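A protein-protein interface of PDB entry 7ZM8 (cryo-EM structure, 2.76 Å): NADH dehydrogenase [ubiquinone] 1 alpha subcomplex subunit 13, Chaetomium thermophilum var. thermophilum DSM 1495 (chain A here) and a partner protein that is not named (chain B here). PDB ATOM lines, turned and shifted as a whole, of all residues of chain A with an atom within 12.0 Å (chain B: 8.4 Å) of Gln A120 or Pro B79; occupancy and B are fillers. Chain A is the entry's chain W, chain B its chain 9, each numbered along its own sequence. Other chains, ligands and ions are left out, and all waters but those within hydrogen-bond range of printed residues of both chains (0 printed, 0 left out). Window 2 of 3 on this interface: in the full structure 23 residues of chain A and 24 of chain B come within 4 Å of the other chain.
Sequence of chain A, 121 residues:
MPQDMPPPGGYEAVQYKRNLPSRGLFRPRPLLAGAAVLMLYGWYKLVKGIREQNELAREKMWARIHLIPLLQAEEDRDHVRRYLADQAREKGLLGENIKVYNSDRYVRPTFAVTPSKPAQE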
ATOM      1  N   PRO A 115     -19.898  -6.749  32.899  1.00  0.00           N
ATOM      2  CA  PRO A 115     -19.621  -6.187  31.591  1.00  0.00           C
ATOM      3  C   PRO A 115     -20.546  -6.850  30.566  1.00  0.00           C
ATOM      4  O   PRO A 115     -20.951  -7.968  30.778  1.00  0.00           O
ATOM      5  CB  PRO A 115     -18.171  -6.583  31.317  1.00  0.00           C
ATOM      6  CG  PRO A 115     -17.569  -6.723  32.683  1.00  0.00           C
ATOM      7  CD  PRO A 115     -18.682  -7.369  33.472  1.00  0.00           C
ATOM      8  N   SER A 116     -20.834  -6.155  29.470  1.00  0.00           N
ATOM      9  CA  SER A 116     -21.750  -6.684  28.429  1.00  0.00           C
ATOM     10  C   SER A 116     -21.184  -7.960  27.805  1.00  0.00           C
ATOM     11  O   SER A 116     -21.986  -8.847  27.485  1.00  0.00           O
ATOM     12  CB  SER A 116     -22.027  -5.630  27.401  1.00  0.00           C
ATOM     13  OG  SER A 116     -20.835  -4.940  27.058  1.00  0.00           O
ATOM     14  N   LYS A 117     -19.866  -8.032  27.606  1.00  0.00           N
ATOM     15  CA  LYS A 117     -19.254  -9.214  26.945  1.00  0.00           C
ATOM     16  C   LYS A 117     -18.072  -9.792  27.742  1.00  0.00           C
ATOM     17  O   LYS A 117     -17.359  -8.999  28.372  1.00  0.00           O
ATOM     18  CB  LYS A 117     -18.745  -8.852  25.546  1.00  0.00           C
ATOM     19  CG  LYS A 117     -19.805  -8.391  24.554  1.00  0.00           C
ATOM     20  CD  LYS A 117     -20.828  -9.457  24.224  1.00  0.00           C
ATOM     21  CE  LYS A 117     -20.246 -10.623  23.455  1.00  0.00           C
ATOM     22  NZ  LYS A 117     -19.722 -10.201  22.135  1.00  0.00           N
ATOM     23  N   PRO A 118     -17.807 -11.127  27.740  1.00  0.00           N
ATOM     24  CA  PRO A 118     -16.617 -11.664  28.387  1.00  0.00           C
ATOM     25  C   PRO A 118     -15.313 -11.367  27.635  1.00  0.00           C
ATOM     26  O   PRO A 118     -15.381 -10.979  26.484  1.00  0.00           O
ATOM     27  CB  PRO A 118     -16.849 -13.168  28.308  1.00  0.00           C
ATOM     28  CG  PRO A 118     -18.329 -13.322  28.088  1.00  0.00           C
ATOM     29  CD  PRO A 118     -18.658 -12.169  27.173  1.00  0.00           C
ATOM     30  N   ALA A 119     -14.164 -11.573  28.285  1.00  0.00           N
ATOM     31  CA  ALA A 119     -12.845 -11.359  27.637  1.00  0.00           C
ATOM     32  C   ALA A 119     -12.720 -12.235  26.385  1.00  0.00           C
ATOM     33  O   ALA A 119     -13.099 -13.417  26.464  1.00  0.00           O
ATOM     34  CB  ALA A 119     -11.744 -11.642  28.623  1.00  0.00           C
ATOM     35  N   GLN A 120     -12.187 -11.686  25.288  1.00  0.00           N
ATOM     36  CA  GLN A 120     -12.110 -12.419  23.990  1.00  0.00           C
ATOM     37  C   GLN A 120     -11.651 -13.873  24.135  1.00  0.00           C
ATOM     38  O   GLN A 120     -12.313 -14.734  23.524  1.00  0.00           O
ATOM     39  CB  GLN A 120     -11.220 -11.662  23.003  1.00  0.00           C
ATOM     40  CG  GLN A 120     -11.944 -10.557  22.246  1.00  0.00           C
ATOM     41  CD  GLN A 120     -12.261  -9.356  23.103  1.00  0.00           C
ATOM     42  OE1 GLN A 120     -13.357  -8.801  23.046  1.00  0.00           O
ATOM     43  NE2 GLN A 120     -11.300  -8.945  23.914  1.00  0.00           N
ATOM     44  N   GLU A 121     -10.548 -14.126  24.846  1.00  0.00           N
ATOM     45  CA  GLU A 121     -10.008 -15.477  25.004  1.00  0.00           C
ATOM     46  C   GLU A 121      -9.561 -16.068  23.670  1.00  0.00           C
ATOM     47  O   GLU A 121      -9.121 -15.346  22.776  1.00  0.00           O
ATOM     48  CB  GLU A 121     -11.039 -16.396  25.664  1.00  0.00           C
ATOM     49  N   GLN B  76     -11.597   2.578  23.750  1.00  0.00           N
ATOM     50  CA  GLN B  76     -10.890   1.438  24.317  1.00  0.00           C
ATOM     51  C   GLN B  76      -9.509   1.339  23.685  1.00  0.00           C
ATOM     52  O   GLN B  76      -9.377   1.388  22.458  1.00  0.00           O
ATOM     53  CB  GLN B  76     -11.677   0.143  24.101  1.00  0.00           C
ATOM     54  CG  GLN B  76     -12.180  -0.065  22.681  1.00  0.00           C
ATOM     55  CD  GLN B  76     -11.227  -0.892  21.841  1.00  0.00           C
ATOM     56  OE1 GLN B  76     -10.436  -1.674  22.368  1.00  0.00           O
ATOM     57  NE2 GLN B  76     -11.300  -0.723  20.527  1.00  0.00           N
ATOM     58  N   GLU B  77      -8.481   1.219  24.525  1.00  0.00           N
ATOM     59  CA  GLU B  77      -7.117   1.137  24.014  1.00  0.00           C
ATOM     60  C   GLU B  77      -6.773  -0.286  23.585  1.00  0.00           C
ATOM     61  O   GLU B  77      -6.524  -0.549  22.404  1.00  0.00           O
ATOM     62  CB  GLU B  77      -6.130   1.632  25.075  1.00  0.00           C
ATOM     63  CG  GLU B  77      -6.600   2.856  25.845  1.00  0.00           C
ATOM     64  CD  GLU B  77      -6.714   4.092  24.976  1.00  0.00           C
ATOM     65  OE1 GLU B  77      -5.921   4.222  24.019  1.00  0.00           O
ATOM     66  OE2 GLU B  77      -7.594   4.934  25.249  1.00  0.00           O
ATOM     67  N   ASN B  78      -6.769  -1.219  24.535  1.00  0.00           N
ATOM     68  CA  ASN B  78      -6.450  -2.616  24.272  1.00  0.00           C
ATOM     69  C   ASN B  78      -7.070  -3.498  25.349  1.00  0.00           C
ATOM     70  O   ASN B  78      -6.522  -3.602  26.454  1.00  0.00           O
ATOM     71  CB  ASN B  78      -4.936  -2.828  24.221  1.00  0.00           C
ATOM     72  CG  ASN B  78      -4.360  -2.586  22.843  1.00  0.00           C
ATOM     73  OD1 ASN B  78      -4.942  -2.987  21.836  1.00  0.00           O
ATOM     74  ND2 ASN B  78      -3.208  -1.927  22.790  1.00  0.00           N
ATOM     75  N   PRO B  79      -8.202  -4.138  25.076  1.00  0.00           N
ATOM     76  CA  PRO B  79      -8.845  -4.978  26.093  1.00  0.00           C
ATOM     77  C   PRO B  79      -7.974  -6.170  26.444  1.00  0.00           C
ATOM     78  O   PRO B  79      -7.368  -6.791  25.558  1.00  0.00           O
ATOM     79  CB  PRO B  79     -10.155  -5.417  25.424  1.00  0.00           C
ATOM     80  CG  PRO B  79      -9.932  -5.254  23.966  1.00  0.00           C
ATOM     81  CD  PRO B  79      -8.845  -4.245  23.756  1.00  0.00           C
ATOM     82  N   PRO B  80      -7.881  -6.518  27.727  1.00  0.00           N
ATOM     83  CA  PRO B  80      -7.033  -7.650  28.126  1.00  0.00           C
ATOM     84  C   PRO B  80      -7.684  -8.976  27.767  1.00  0.00           C
ATOM     85  O   PRO B  80      -8.866  -9.197  28.034  1.00  0.00           O
ATOM     86  CB  PRO B  80      -6.904  -7.481  29.645  1.00  0.00           C
ATOM     87  CG  PRO B  80      -7.422  -6.094  29.943  1.00  0.00           C
ATOM     88  CD  PRO B  80      -8.433  -5.809  28.890  1.00  0.00           C
ATOM     89  N   THR B  81      -6.900  -9.863  27.160  1.00  0.00           N
ATOM     90  CA  THR B  81      -7.404 -11.184  26.827  1.00  0.00           C
ATOM     91  C   THR B  81      -7.629 -11.993  28.097  1.00  0.00           C
ATOM     92  O   THR B  81      -7.141 -11.651  29.176  1.00  0.00           O
ATOM     93  CB  THR B  81      -6.435 -11.914  25.895  1.00  0.00           C
ATOM     94  OG1 THR B  81      -7.009 -13.163  25.491  1.00  0.00           O
ATOM     95  CG2 THR B  81      -5.114 -12.175  26.592  1.00  0.00           C
ATOM     96  N   ALA B  82      -8.403 -13.072  27.972  1.00  0.00           N
ATOM     97  CA  ALA B  82      -8.712 -13.856  29.184  1.00  0.00           C
ATOM     98  C   ALA B  82      -7.421 -14.491  29.700  1.00  0.00           C
ATOM     99  O   ALA B  82      -7.246 -14.525  30.923  1.00  0.00           O
ATOM    100  CB  ALA B  82      -9.779 -14.882  28.900  1.00  0.00           C
ATOM    101  N   GLY B  83      -6.576 -15.008  28.809  1.00  0.00           N
ATOM    102  CA  GLY B  83      -5.345 -15.622  29.276  1.00  0.00           C
ATOM    103  C   GLY B  83      -4.483 -14.660  30.066  1.00  0.00           C
ATOM    104  O   GLY B  83      -3.782 -15.059  30.998  1.00  0.00           O
ATOM    105  N   GLN B  84      -4.506 -13.382  29.690  1.00  0.00           N
ATOM    106  CA  GLN B  84      -3.827 -12.369  30.486  1.00  0.00           C
ATOM    107  C   GLN B  84      -4.452 -12.248  31.870  1.00  0.00           C
ATOM    108  O   GLN B  84      -3.740 -12.080  32.866  1.00  0.00           O
ATOM    109  CB  GLN B  84      -3.859 -11.028  29.760  1.00  0.00           C
ATOM    110  CG  GLN B  84      -2.608 -10.736  28.960  1.00  0.00           C
ATOM    111  CD  GLN B  84      -2.824  -9.667  27.911  1.00  0.00           C
ATOM    112  OE1 GLN B  84      -3.935  -9.170  27.734  1.00  0.00           O
ATOM    113  NE2 GLN B  84      -1.757  -9.305  27.208  1.00  0.00           N
ATOM    114  N   ILE B  85      -5.789 -12.327  31.955  1.00  0.00           N
ATOM    115  CA  ILE B  85      -6.507 -12.156  33.259  1.00  0.00           C
ATOM    116  C   ILE B  85      -6.635 -13.519  33.944  1.00  0.00           C
ATOM    117  O   ILE B  85      -7.521 -13.664  34.796  1.00  0.00           O
ATOM    118  CB  ILE B  85      -7.882 -11.470  33.092  1.00  0.00           C
ATOM    119  CG1 ILE B  85      -7.929 -10.541  31.880  1.00  0.00           C
ATOM    120  CG2 ILE B  85      -8.273 -10.727  34.360  1.00  0.00           C
ATOM    121  CD1 ILE B  85      -9.311 -10.029  31.564  1.00  0.00           C
ATOM    122  N   ARG B  86      -5.816 -14.494  33.551  1.00  0.00           N
ATOM    123  CA  ARG B  86      -5.788 -15.816  34.226  1.00  0.00           C
ATOM    124  C   ARG B  86      -4.371 -15.911  34.775  1.00  0.00           C
ATOM    125  O   ARG B  86      -4.094 -16.811  35.585  1.00  0.00           O
ATOM    126  CB  ARG B  86      -6.132 -16.927  33.233  1.00  0.00           C
ATOM    127  CG  ARG B  86      -7.166 -17.917  33.749  1.00  0.00           C
ATOM    128  CD  ARG B  86      -7.521 -18.977  32.725  1.00  0.00           C
ATOM    129  NE  ARG B  86      -8.318 -18.475  31.617  1.00  0.00           N
ATOM    130  CZ  ARG B  86      -9.644 -18.434  31.612  1.00  0.00           C
ATOM    131  NH1 ARG B  86     -10.319 -18.852  32.668  1.00  0.00           N
ATOM    132  NH2 ARG B  86     -10.292 -17.972  30.559  1.00  0.00           N
ATOM    133  N   LYS B  99      -0.563  -5.206  33.077  1.00  0.00           N
ATOM    134  CA  LYS B  99      -1.509  -4.918  32.004  1.00  0.00           C
ATOM    135  C   LYS B  99      -2.947  -5.002  32.497  1.00  0.00           C
ATOM    136  O   LYS B  99      -3.786  -4.175  32.125  1.00  0.00           O
ATOM    137  CB  LYS B  99      -1.283  -5.872  30.834  1.00  0.00           C
ATOM    138  CG  LYS B  99      -2.181  -5.603  29.644  1.00  0.00           C
ATOM    139  CD  LYS B  99      -1.934  -4.216  29.078  1.00  0.00           C
ATOM    140  CE  LYS B  99      -0.561  -4.116  28.437  1.00  0.00           C
ATOM    141  NZ  LYS B  99      -0.323  -2.766  27.855  1.00  0.00           N
ATOM    142  N   VAL B 100      -3.254  -6.000  33.326  1.00  0.00           N
ATOM    143  CA  VAL B 100      -4.594  -6.109  33.889  1.00  0.00           C
ATOM    144  C   VAL B 100      -4.894  -4.905  34.769  1.00  0.00           C
ATOM    145  O   VAL B 100      -5.985  -4.327  34.717  1.00  0.00           O
ATOM    146  CB  VAL B 100      -4.745  -7.432  34.663  1.00  0.00           C
ATOM    147  CG1 VAL B 100      -6.045  -7.452  35.442  1.00  0.00           C
ATOM    148  CG2 VAL B 100      -4.693  -8.614  33.711  1.00  0.00           C
ATOM    149  N   CYS B 102      -3.351  -1.999  34.583  1.00  0.00           N
ATOM    150  CA  CYS B 102      -3.167  -0.767  33.817  1.00  0.00           C
ATOM    151  C   CYS B 102      -2.459   0.301  34.648  1.00  0.00           C
ATOM    152  O   CYS B 102      -2.804   1.484  34.608  1.00  0.00           O
ATOM    153  CB  CYS B 102      -4.504  -0.252  33.284  1.00  0.00           C
ATOM    154  SG  CYS B 102      -5.469  -1.507  32.414  1.00  0.00           S
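OE1 of Gln B84 is in hydrogen-bond range of N of Thr B81 (3.1 Å).
O of Pro B80 touches CB of Ala A119, at 3.8 Å. Ala A119 touches Ala B82. Pro B79 touches Gln A120 (CG to NE2, 3.9 Å). OG1 of Thr B81 touches N of Glu A121, at 3.7 Å. CB of Ala B82 touches CB of Glu A121, at 3.8 Å.
Pro A118 touches none of the printed residues of chain B. Ala A119 touches just these residues of chain B: Pro B80 and Ala B82. Of the printed residues of chain B, Gln A120 touches Pro B79. Glu A121 touches just these residues of chain B: Thr B81 and Ala B82. No residue of chain A comes within 4 Å of Gln B76. Glu B77 touches none of the printed residues of chain A. Pro B79 touches one residue of chain A. Pro B80 touches just one residue of chain A: Ala A119. Thr B81 touches one residue of chain A. Printed residues of chain A within 4 Å of Ala B82: Ala A119 (3.7 Å) and Glu A121 (3.8 Å). The nearest residue of chain B that does not touch Gln A120 is Pro B80 (4.8 Å). The nearest printed residue of chain A that does not touch Ala B82 is Gln A120 (4.8 Å).
Of the 14 printed residues of chain B, 4 touch a printed residue of chain A. Printed residues of chain B that touch a printed residue of chain A: Pro B79, Pro B80, Thr B81 and Ala B82. Hydrophobic or aromatic side chains of chain B that line the printed part of chain A: Pro B79 and Ala B82. Along chain B the printed residues that touch a printed residue of chain A span positions 79 to 82. Printed residues of chain A that touch a printed residue of chain B: Ala A119, Gln A120 and Glu A121. Among the printed residues, 5 pairs touch across the chains. Among the printed residues, no Asp or Glu carboxylate lies within 4 Å of a Lys or Arg side-chain nitrogen of the other chain.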
